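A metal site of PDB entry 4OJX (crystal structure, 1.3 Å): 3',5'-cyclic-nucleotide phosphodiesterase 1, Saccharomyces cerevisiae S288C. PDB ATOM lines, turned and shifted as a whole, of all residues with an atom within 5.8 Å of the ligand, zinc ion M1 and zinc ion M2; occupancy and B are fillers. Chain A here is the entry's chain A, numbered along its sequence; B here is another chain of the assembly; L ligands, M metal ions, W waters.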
ATOM      1  N   GLY A  13      15.484 -23.730 -17.598  1.00  0.00           N
ATOM      2  CA  GLY A  13      14.077 -24.036 -17.824  1.00  0.00           C
ATOM      3  C   GLY A  13      13.096 -23.288 -16.942  1.00  0.00           C
ATOM      4  O   GLY A  13      11.895 -23.447 -17.105  1.00  0.00           O
ATOM      5  N   GLN A  21      15.893 -19.930 -22.398  1.00  0.00           N
ATOM      6  CA  GLN A  21      16.410 -20.577 -23.601  1.00  0.00           C
ATOM      7  C   GLN A  21      16.779 -19.629 -24.746  1.00  0.00           C
ATOM      8  O   GLN A  21      15.921 -18.916 -25.283  1.00  0.00           O
ATOM      9  CB  GLN A  21      15.417 -21.619 -24.102  1.00  0.00           C
ATOM     10  CG  GLN A  21      15.945 -22.383 -25.309  1.00  0.00           C
ATOM     11  CD  GLN A  21      15.380 -23.780 -25.401  1.00  0.00           C
ATOM     12  OE1 GLN A  21      15.522 -24.580 -24.483  1.00  0.00           O
ATOM     13  NE2 GLN A  21      14.760 -24.092 -26.529  1.00  0.00           N
ATOM     14  N   HIS A 128       8.495 -21.781 -29.758  1.00  0.00           N
ATOM     15  CA  HIS A 128       7.137 -21.569 -29.273  1.00  0.00           C
ATOM     16  C   HIS A 128       7.119 -20.281 -28.503  1.00  0.00           C
ATOM     17  O   HIS A 128       8.177 -19.812 -28.073  1.00  0.00           O
ATOM     18  CB  HIS A 128       6.627 -22.771 -28.472  1.00  0.00           C
ATOM     19  CG  HIS A 128       7.277 -22.976 -27.104  1.00  0.00           C
ATOM     20  ND1 HIS A 128       8.587 -23.266 -26.937  1.00  0.00           N
ATOM     21  CD2 HIS A 128       6.705 -22.994 -25.841  1.00  0.00           C
ATOM     22  CE1 HIS A 128       8.838 -23.453 -25.617  1.00  0.00           C
ATOM     23  NE2 HIS A 128       7.688 -23.296 -24.943  1.00  0.00           N
ATOM     24  N   HIS A 130       5.987 -19.260 -25.533  1.00  0.00           N
ATOM     25  CA  HIS A 130       6.046 -19.105 -24.073  1.00  0.00           C
ATOM     26  C   HIS A 130       7.062 -18.053 -23.714  1.00  0.00           C
ATOM     27  O   HIS A 130       8.131 -17.959 -24.344  1.00  0.00           O
ATOM     28  CB  HIS A 130       6.415 -20.404 -23.376  1.00  0.00           C
ATOM     29  CG  HIS A 130       5.245 -21.348 -23.199  1.00  0.00           C
ATOM     30  ND1 HIS A 130       5.428 -22.669 -22.948  1.00  0.00           N
ATOM     31  CD2 HIS A 130       3.879 -21.120 -23.209  1.00  0.00           C
ATOM     32  CE1 HIS A 130       4.229 -23.254 -22.811  1.00  0.00           C
ATOM     33  NE2 HIS A 130       3.285 -22.309 -22.973  1.00  0.00           N
ATOM     34  N   ASP A 132       9.356 -17.426 -21.573  1.00  0.00           N
ATOM     35  CA  ASP A 132      10.772 -17.751 -21.326  1.00  0.00           C
ATOM     36  C   ASP A 132      11.572 -17.920 -22.613  1.00  0.00           C
ATOM     37  O   ASP A 132      12.809 -17.860 -22.577  1.00  0.00           O
ATOM     38  CB  ASP A 132      10.977 -18.955 -20.376  1.00  0.00           C
ATOM     39  CG  ASP A 132      10.292 -20.240 -20.858  1.00  0.00           C
ATOM     40  OD1 ASP A 132       9.088 -20.125 -21.186  1.00  0.00           O
ATOM     41  OD2 ASP A 132      10.925 -21.366 -20.913  1.00  0.00           O
ATOM     42  N   HIS A 133      10.893 -18.110 -23.751  1.00  0.00           N
ATOM     43  CA  HIS A 133      11.561 -18.295 -25.041  1.00  0.00           C
ATOM     44  C   HIS A 133      11.576 -17.056 -25.871  1.00  0.00           C
ATOM     45  O   HIS A 133      12.125 -17.082 -26.972  1.00  0.00           O
ATOM     46  CB  HIS A 133      10.969 -19.482 -25.806  1.00  0.00           C
ATOM     47  CG  HIS A 133      11.142 -20.773 -25.069  1.00  0.00           C
ATOM     48  ND1 HIS A 133      12.026 -21.737 -25.432  1.00  0.00           N
ATOM     49  CD2 HIS A 133      10.554 -21.203 -23.907  1.00  0.00           C
ATOM     50  CE1 HIS A 133      11.988 -22.721 -24.519  1.00  0.00           C
ATOM     51  NE2 HIS A 133      11.105 -22.387 -23.584  1.00  0.00           N
ATOM     52  N   HIS A 213       3.728 -30.065 -26.695  1.00  0.00           N
ATOM     53  CA  HIS A 213       4.276 -29.435 -25.493  1.00  0.00           C
ATOM     54  C   HIS A 213       3.170 -29.186 -24.491  1.00  0.00           C
ATOM     55  O   HIS A 213       3.018 -28.108 -23.938  1.00  0.00           O
ATOM     56  CB  HIS A 213       5.028 -28.177 -25.916  1.00  0.00           C
ATOM     57  CG  HIS A 213       5.580 -27.331 -24.783  1.00  0.00           C
ATOM     58  ND1 HIS A 213       6.009 -27.843 -23.619  1.00  0.00           N
ATOM     59  CD2 HIS A 213       5.769 -25.948 -24.697  1.00  0.00           C
ATOM     60  CE1 HIS A 213       6.419 -26.849 -22.806  1.00  0.00           C
ATOM     61  NE2 HIS A 213       6.287 -25.693 -23.473  1.00  0.00           N
ATOM     62  N   ILE A 215      -0.774 -29.222 -22.715  1.00  0.00           N
ATOM     63  CA  ILE A 215      -2.126 -28.760 -23.021  1.00  0.00           C
ATOM     64  C   ILE A 215      -2.430 -27.497 -22.234  1.00  0.00           C
ATOM     65  O   ILE A 215      -1.845 -27.251 -21.172  1.00  0.00           O
ATOM     66  CB  ILE A 215      -3.207 -29.845 -22.736  1.00  0.00           C
ATOM     67  CG1 ILE A 215      -3.167 -30.284 -21.263  1.00  0.00           C
ATOM     68  CG2 ILE A 215      -3.056 -31.032 -23.686  1.00  0.00           C
ATOM     69  CD1 ILE A 215      -4.351 -31.118 -20.820  1.00  0.00           C
ATOM     70  N   VAL A 217      -4.106 -25.010 -19.678  1.00  0.00           N
ATOM     71  CA  VAL A 217      -4.717 -25.176 -18.364  1.00  0.00           C
ATOM     72  C   VAL A 217      -6.216 -24.914 -18.417  1.00  0.00           C
ATOM     73  O   VAL A 217      -7.013 -25.715 -17.923  1.00  0.00           O
ATOM     74  CB  VAL A 217      -4.056 -24.224 -17.337  1.00  0.00           C
ATOM     75  CG1 VAL A 217      -4.713 -24.367 -15.970  1.00  0.00           C
ATOM     76  CG2 VAL A 217      -2.558 -24.464 -17.259  1.00  0.00           C
ATOM     77  N   ASP A 244      10.691 -26.868 -26.265  1.00  0.00           N
ATOM     78  CA  ASP A 244      10.126 -27.668 -25.169  1.00  0.00           C
ATOM     79  C   ASP A 244       9.233 -28.752 -25.786  1.00  0.00           C
ATOM     80  O   ASP A 244       8.563 -28.500 -26.807  1.00  0.00           O
ATOM     81  CB  ASP A 244       9.256 -26.825 -24.191  1.00  0.00           C
ATOM     82  CG  ASP A 244       9.984 -25.613 -23.524  1.00  0.00           C
ATOM     83  OD1 ASP A 244      11.228 -25.537 -23.827  1.00  0.00           O
ATOM     84  OD2 ASP A 244       9.285 -24.763 -22.766  1.00  0.00           O
ATOM     85  N   SER A 281      13.719 -31.315 -18.713  1.00  0.00           N
ATOM     86  CA  SER A 281      13.387 -30.312 -17.695  1.00  0.00           C
ATOM     87  C   SER A 281      13.472 -30.841 -16.275  1.00  0.00           C
ATOM     88  O   SER A 281      13.830 -30.107 -15.367  1.00  0.00           O
ATOM     89  CB  SER A 281      11.985 -29.742 -17.912  1.00  0.00           C
ATOM     90  OG  SER A 281      11.899 -28.969 -19.087  1.00  0.00           O
ATOM     91  N   GLU A 289       3.347 -31.672 -11.538  1.00  0.00           N
ATOM     92  CA  GLU A 289       3.121 -30.270 -11.904  1.00  0.00           C
ATOM     93  C   GLU A 289       4.268 -29.640 -12.696  1.00  0.00           C
ATOM     94  O   GLU A 289       4.025 -28.869 -13.633  1.00  0.00           O
ATOM     95  CB  GLU A 289       2.832 -29.422 -10.657  1.00  0.00           C
ATOM     96  CG  GLU A 289       1.478 -29.681  -9.995  1.00  0.00           C
ATOM     97  CD  GLU A 289       1.427 -30.986  -9.231  1.00  0.00           C
ATOM     98  OE1 GLU A 289       2.434 -31.354  -8.595  1.00  0.00           O
ATOM     99  OE2 GLU A 289       0.361 -31.654  -9.258  1.00  0.00           O
ATOM    100  N   GLN A 290       5.506 -29.970 -12.331  1.00  0.00           N
ATOM    101  CA  GLN A 290       6.681 -29.426 -13.000  1.00  0.00           C
ATOM    102  C   GLN A 290       6.971 -30.135 -14.336  1.00  0.00           C
ATOM    103  O   GLN A 290       7.580 -29.546 -15.232  1.00  0.00           O
ATOM    104  CB  GLN A 290       7.908 -29.477 -12.090  1.00  0.00           C
ATOM    105  CG  GLN A 290       8.897 -28.346 -12.345  1.00  0.00           C
ATOM    106  CD  GLN A 290      10.206 -28.475 -11.564  1.00  0.00           C
ATOM    107  OE1 GLN A 290      10.724 -29.577 -11.377  1.00  0.00           O
ATOM    108  NE2 GLN A 290      10.747 -27.347 -11.136  1.00  0.00           N
ATOM    109  N   LEU A 291       6.511 -31.377 -14.452  1.00  0.00           N
ATOM    110  CA  LEU A 291       6.779 -32.212 -15.630  1.00  0.00           C
ATOM    111  C   LEU A 291       5.835 -31.994 -16.821  1.00  0.00           C
ATOM    112  O   LEU A 291       6.207 -32.299 -17.961  1.00  0.00           O
ATOM    113  CB  LEU A 291       6.823 -33.705 -15.237  1.00  0.00           C
ATOM    114  CG  LEU A 291       7.224 -34.749 -16.286  1.00  0.00           C
ATOM    115  CD1 LEU A 291       8.659 -34.519 -16.770  1.00  0.00           C
ATOM    116  CD2 LEU A 291       7.064 -36.158 -15.738  1.00  0.00           C
ATOM    117  N   TYR A 292       4.643 -31.458 -16.575  1.00  0.00           N
ATOM    118  CA  TYR A 292       3.650 -31.218 -17.641  1.00  0.00           C
ATOM    119  C   TYR A 292       4.191 -30.474 -18.877  1.00  0.00           C
ATOM    120  O   TYR A 292       4.661 -29.334 -18.785  1.00  0.00           O
ATOM    121  CB  TYR A 292       2.410 -30.494 -17.102  1.00  0.00           C
ATOM    122  CG  TYR A 292       1.592 -31.267 -16.077  1.00  0.00           C
ATOM    123  CD1 TYR A 292       1.020 -30.613 -14.990  1.00  0.00           C
ATOM    124  CD2 TYR A 292       1.389 -32.653 -16.204  1.00  0.00           C
ATOM    125  CE1 TYR A 292       0.268 -31.306 -14.053  1.00  0.00           C
ATOM    126  CE2 TYR A 292       0.637 -33.346 -15.268  1.00  0.00           C
ATOM    127  CZ  TYR A 292       0.084 -32.671 -14.196  1.00  0.00           C
ATOM    128  OH  TYR A 292      -0.666 -33.355 -13.264  1.00  0.00           O
ATOM    129  N   HIS A 294       6.724 -31.582 -20.700  1.00  0.00           N
ATOM    130  CA  HIS A 294       8.188 -31.704 -20.728  1.00  0.00           C
ATOM    131  C   HIS A 294       8.642 -33.123 -20.679  1.00  0.00           C
ATOM    132  O   HIS A 294       7.822 -34.051 -20.583  1.00  0.00           O
ATOM    133  CB  HIS A 294       8.785 -30.940 -19.553  1.00  0.00           C
ATOM    134  CG  HIS A 294       8.621 -29.456 -19.652  1.00  0.00           C
ATOM    135  ND1 HIS A 294       9.158 -28.727 -20.647  1.00  0.00           N
ATOM    136  CD2 HIS A 294       7.931 -28.561 -18.840  1.00  0.00           C
ATOM    137  CE1 HIS A 294       8.832 -27.447 -20.485  1.00  0.00           C
ATOM    138  NE2 HIS A 294       8.080 -27.345 -19.372  1.00  0.00           N
ATOM    139  N   HIS A 326      17.291 -26.712 -20.842  1.00  0.00           N
ATOM    140  CA  HIS A 326      16.016 -26.382 -20.200  1.00  0.00           C
ATOM    141  C   HIS A 326      15.807 -27.105 -18.894  1.00  0.00           C
ATOM    142  O   HIS A 326      14.670 -27.412 -18.525  1.00  0.00           O
ATOM    143  CB  HIS A 326      14.876 -26.644 -21.190  1.00  0.00           C
ATOM    144  CG  HIS A 326      13.609 -25.865 -20.917  1.00  0.00           C
ATOM    145  ND1 HIS A 326      12.649 -26.290 -20.066  1.00  0.00           N
ATOM    146  CD2 HIS A 326      13.137 -24.681 -21.474  1.00  0.00           C
ATOM    147  CE1 HIS A 326      11.636 -25.411 -20.062  1.00  0.00           C
ATOM    148  NE2 HIS A 326      11.933 -24.428 -20.915  1.00  0.00           N
ATOM    149  N   LYS A 328      15.086 -27.395 -15.177  1.00  0.00           N
ATOM    150  CA  LYS A 328      14.433 -26.507 -14.234  1.00  0.00           C
ATOM    151  C   LYS A 328      15.139 -26.484 -12.880  1.00  0.00           C
ATOM    152  O   LYS A 328      15.730 -27.495 -12.450  1.00  0.00           O
ATOM    153  CB  LYS A 328      12.979 -26.940 -14.065  1.00  0.00           C
ATOM    154  CG  LYS A 328      12.141 -26.581 -15.286  1.00  0.00           C
ATOM    155  CD  LYS A 328      10.685 -27.000 -15.138  1.00  0.00           C
ATOM    156  CE  LYS A 328       9.875 -26.619 -16.369  1.00  0.00           C
ATOM    157  NZ  LYS A 328       9.749 -25.144 -16.593  1.00  0.00           N
ATOM    158  N   PRO B 142       5.398 -20.507 -11.662  1.00  0.00           N
ATOM    159  CA  PRO B 142       5.184 -21.932 -11.328  1.00  0.00           C
ATOM    160  C   PRO B 142       5.755 -22.344  -9.968  1.00  0.00           C
ATOM    161  O   PRO B 142       5.366 -23.404  -9.461  1.00  0.00           O
ATOM    162  CB  PRO B 142       5.873 -22.663 -12.478  1.00  0.00           C
ATOM    163  CG  PRO B 142       5.835 -21.689 -13.605  1.00  0.00           C
ATOM    164  CD  PRO B 142       6.077 -20.361 -12.958  1.00  0.00           C
ATOM    165  N   TYR B 145       3.572 -23.719  -7.070  1.00  0.00           N
ATOM    166  CA  TYR B 145       3.137 -25.115  -6.991  1.00  0.00           C
ATOM    167  C   TYR B 145       4.122 -26.087  -6.338  1.00  0.00           C
ATOM    168  O   TYR B 145       3.877 -27.299  -6.322  1.00  0.00           O
ATOM    169  CB  TYR B 145       2.746 -25.618  -8.376  1.00  0.00           C
ATOM    170  CG  TYR B 145       1.691 -24.775  -9.028  1.00  0.00           C
ATOM    171  CD1 TYR B 145       0.400 -24.730  -8.505  1.00  0.00           C
ATOM    172  CD2 TYR B 145       1.991 -23.992 -10.127  1.00  0.00           C
ATOM    173  CE1 TYR B 145      -0.578 -23.943  -9.090  1.00  0.00           C
ATOM    174  CE2 TYR B 145       1.028 -23.200 -10.719  1.00  0.00           C
ATOM    175  CZ  TYR B 145      -0.255 -23.178 -10.192  1.00  0.00           C
ATOM    176  OH  TYR B 145      -1.218 -22.386 -10.785  1.00  0.00           O
ATOM    177  N   TRP B 175       1.665 -17.972 -21.815  1.00  0.00           N
ATOM    178  CA  TRP B 175       1.961 -18.638 -20.566  1.00  0.00           C
ATOM    179  C   TRP B 175       0.797 -19.516 -20.237  1.00  0.00           C
ATOM    180  O   TRP B 175      -0.344 -19.139 -20.522  1.00  0.00           O
ATOM    181  CB  TRP B 175       2.162 -17.642 -19.432  1.00  0.00           C
ATOM    182  CG  TRP B 175       2.978 -18.211 -18.315  1.00  0.00           C
ATOM    183  CD1 TRP B 175       2.591 -18.443 -17.008  1.00  0.00           C
ATOM    184  CD2 TRP B 175       4.369 -18.640 -18.392  1.00  0.00           C
ATOM    185  NE1 TRP B 175       3.627 -18.978 -16.277  1.00  0.00           N
ATOM    186  CE2 TRP B 175       4.722 -19.129 -17.067  1.00  0.00           C
ATOM    187  CE3 TRP B 175       5.308 -18.675 -19.405  1.00  0.00           C
ATOM    188  CZ2 TRP B 175       5.995 -19.594 -16.783  1.00  0.00           C
ATOM    189  CZ3 TRP B 175       6.590 -19.162 -19.118  1.00  0.00           C
ATOM    190  CH2 TRP B 175       6.917 -19.606 -17.829  1.00  0.00           C
ATOM    191  N   PRO B 176       1.046 -20.683 -19.608  1.00  0.00           N
ATOM    192  CA  PRO B 176      -0.100 -21.442 -19.102  1.00  0.00           C
ATOM    193  C   PRO B 176      -0.994 -20.575 -18.235  1.00  0.00           C
ATOM    194  O   PRO B 176      -0.496 -19.726 -17.474  1.00  0.00           O
ATOM    195  CB  PRO B 176       0.574 -22.561 -18.291  1.00  0.00           C
ATOM    196  CG  PRO B 176       1.877 -22.774 -19.010  1.00  0.00           C
ATOM    197  CD  PRO B 176       2.325 -21.372 -19.346  1.00  0.00           C
ATOM    198  N   LEU B 178      -2.375 -19.979 -15.367  1.00  0.00           N
ATOM    199  CA  LEU B 178      -2.313 -20.431 -13.988  1.00  0.00           C
ATOM    200  C   LEU B 178      -3.458 -19.863 -13.169  1.00  0.00           C
ATOM    201  O   LEU B 178      -3.799 -20.431 -12.135  1.00  0.00           O
ATOM    202  CB  LEU B 178      -0.957 -20.099 -13.355  1.00  0.00           C
ATOM    203  CG  LEU B 178       0.244 -20.732 -14.062  1.00  0.00           C
ATOM    204  CD1 LEU B 178       1.510 -20.358 -13.309  1.00  0.00           C
ATOM    205  CD2 LEU B 178       0.122 -22.245 -14.180  1.00  0.00           C
ATOM    206  N   GLU B 181      -6.305 -22.530 -12.767  1.00  0.00           N
ATOM    207  CA  GLU B 181      -6.100 -23.639 -11.832  1.00  0.00           C
ATOM    208  C   GLU B 181      -7.070 -23.480 -10.656  1.00  0.00           C
ATOM    209  O   GLU B 181      -7.177 -22.403 -10.081  1.00  0.00           O
ATOM    210  CB  GLU B 181      -4.646 -23.666 -11.350  1.00  0.00           C
ATOM    211  CG  GLU B 181      -4.352 -24.569 -10.154  1.00  0.00           C
ATOM    212  CD  GLU B 181      -4.245 -26.032 -10.539  1.00  0.00           C
ATOM    213  OE1 GLU B 181      -5.269 -26.636 -10.928  1.00  0.00           O
ATOM    214  OE2 GLU B 181      -3.127 -26.578 -10.444  1.00  0.00           O
HETATM  215  P1  LIG L   1       7.786 -24.108 -19.579  1.00  0.00           P
HETATM  216  O1  LIG L   1       7.733 -25.080 -18.471  1.00  0.00           O
HETATM  217  O2  LIG L   1       7.005 -24.533 -20.794  1.00  0.00           O
HETATM  218  O3  LIG L   1       9.212 -23.714 -19.875  1.00  0.00           O
HETATM  219  O4  LIG L   1       7.042 -22.862 -18.963  1.00  0.00           O
HETATM  220  C1  LIG L   1       5.654 -23.035 -18.526  1.00  0.00           C
HETATM  221  C2  LIG L   1       5.444 -23.397 -17.014  1.00  0.00           C
HETATM  222  O5  LIG L   1       4.023 -23.545 -16.741  1.00  0.00           O
HETATM  223  C3  LIG L   1       6.041 -24.757 -16.658  1.00  0.00           C
HETATM  224  O6  LIG L   1       7.187 -24.566 -15.823  1.00  0.00           O
HETATM  225  C4  LIG L   1       4.989 -25.564 -15.910  1.00  0.00           C
HETATM  226  O7  LIG L   1       5.470 -25.908 -14.593  1.00  0.00           O
HETATM  227  C5  LIG L   1       3.804 -24.620 -15.776  1.00  0.00           C
HETATM  228  N1  LIG L   1       2.513 -25.336 -16.054  1.00  0.00           N
HETATM  229  C6  LIG L   1       2.073 -25.611 -17.280  1.00  0.00           C
HETATM  230  N2  LIG L   1       0.898 -26.237 -17.171  1.00  0.00           N
HETATM  231  C7  LIG L   1       0.612 -26.346 -15.884  1.00  0.00           C
HETATM  232  C8  LIG L   1      -0.443 -26.893 -15.257  1.00  0.00           C
HETATM  233  O8  LIG L   1      -1.356 -27.412 -15.900  1.00  0.00           O
HETATM  234  N3  LIG L   1      -0.501 -26.895 -13.862  1.00  0.00           N
HETATM  235  C9  LIG L   1       0.550 -26.303 -13.157  1.00  0.00           C
HETATM  236  N4  LIG L   1       0.502 -26.292 -11.827  1.00  0.00           N
HETATM  237  N5  LIG L   1       1.581 -25.769 -13.826  1.00  0.00           N
HETATM  238  C10 LIG L   1       1.619 -25.789 -15.181  1.00  0.00           C
HETATM  239 ZN    ZN M   1      10.428 -23.266 -21.793  1.00  0.00          ZN
HETATM  240 ZN    ZN M   2       7.241 -23.859 -22.900  1.00  0.00          ZN
HETATM  241  O   HOH W   1      -1.477 -28.061 -18.573  1.00  0.00           O
HETATM  242  O   HOH W   2       8.921 -23.822 -14.268  1.00  0.00           O
HETATM  243  O   HOH W   3       8.542 -22.605 -22.038  1.00  0.00           O
HETATM  244  O   HOH W   4       4.671 -26.021 -20.041  1.00  0.00           O
HETATM  245  O   HOH W   5       9.786 -21.581 -17.778  1.00  0.00           O
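Four residues have an atom within 4 Å of zinc ion M2: His 128, His 130, His 213 and Asp 244.
A ring nitrogen (NE2) of His 294 sits at hydrogen-bond distance from an oxygen (O1) of the ligand (2.5 Å).
O of Glu 289 lies within hydrogen-bond range of O7 of the ligand (3.4 Å).
The side-chain amino group of Lys 328 lies within salt-bridge range of an oxygen (O1) of the ligand (2.8 Å).
ND1 of His 294 is in hydrogen-bond range of OG of Ser 281, 3.2 Å away.
ND1 of His 326 is in hydrogen-bond range of OG of Ser 281 (2.9 Å).
NZ of Lys 328 is in hydrogen-bond range of O of Gly 13 (2.8 Å).
The backbone NH (N) of Lys 328 is in hydrogen-bond range of the backbone carbonyl oxygen (O) of Ser 281, at 3.0 Å.
Zinc ion M1 is bound by water W3 (2.0 Å).
NE2 of His 326 is bound to zinc ion M1 (2.1 Å).
Zinc ion M1 is bound by NE2 of His 133 (2.1 Å).
OD2 of Asp 244 binds zinc ion M1 (2.1 Å).
Zinc ion M1 is bound by OD2 of Asp 132 (2.2 Å).
An oxygen (O3) of the ligand binds zinc ion M1 (2.3 Å).
Gly 13 touches the ligand (O to O3, 3.9 Å).
Val 217 touches the ligand (CG2 to O8, 3.5 Å).
Pro 142 of chain B touches the ligand.
Tyr 145 of chain B touches the ligand (CD2 to N4, 3.2 Å).
Trp 175 of chain B touches the ligand.
Pro 176 of chain B touches the ligand.
Leu 178 of chain B touches the ligand (CD2 to N5, 3.8 Å).
Glu 181 of chain B touches the ligand.
Hydrophobic or aromatic side chains within 4 Å of the ligand: His 130, His 213, Val 217, His 294, His 326, Pro 142 of chain B, Tyr 145 of chain B, Trp 175 of chain B, Pro 176 of chain B and Leu 178 of chain B.
16 residues have an atom within 4 Å of the ligand: Gly 13, His 130, Asp 132, His 213, Val 217, Asp 244, Glu 289, His 294, His 326, Lys 328, Pro 142 of chain B, Tyr 145 of chain B, Trp 175 of chain B, Pro 176 of chain B, Leu 178 of chain B and Glu 181 of chain B.
The nearest printed residue that does not touch the ligand is Tyr 292 (4.01 Å).
Within 4 Å of zinc ion M1: Asp 132, His 133, Asp 244 and His 326.
Water W3 is bound to zinc ion M2.
NE2 of His 213 is bound to zinc ion M2.
NE2 of His 128 binds zinc ion M2 (2.2 Å).
A ring nitrogen (ND1) of His 130 binds zinc ion M2.
Zinc ion M2 is bound by O2 of the ligand, at 2.2 Å.
Zinc ion M2 is bound by OD2 of Asp 244.
Zinc ion M2 has six donor atoms within binding distance.
Water W3 lies within hydrogen-bond range of OD1 of Asp 132 and O4 of the ligand.
Water W2 bridges O6 of the ligand (2.4 Å) and NZ of Lys 328 (2.8 Å).
Water W1 lies within hydrogen-bond range of the backbone carbonyl oxygen of Ile 215 (2.7 Å) and an oxygen (O8) of the ligand (2.8 Å).
Water W5 lies within hydrogen-bond range of O of Gly 13 (2.9 Å) and O4 of the ligand (3.3 Å).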
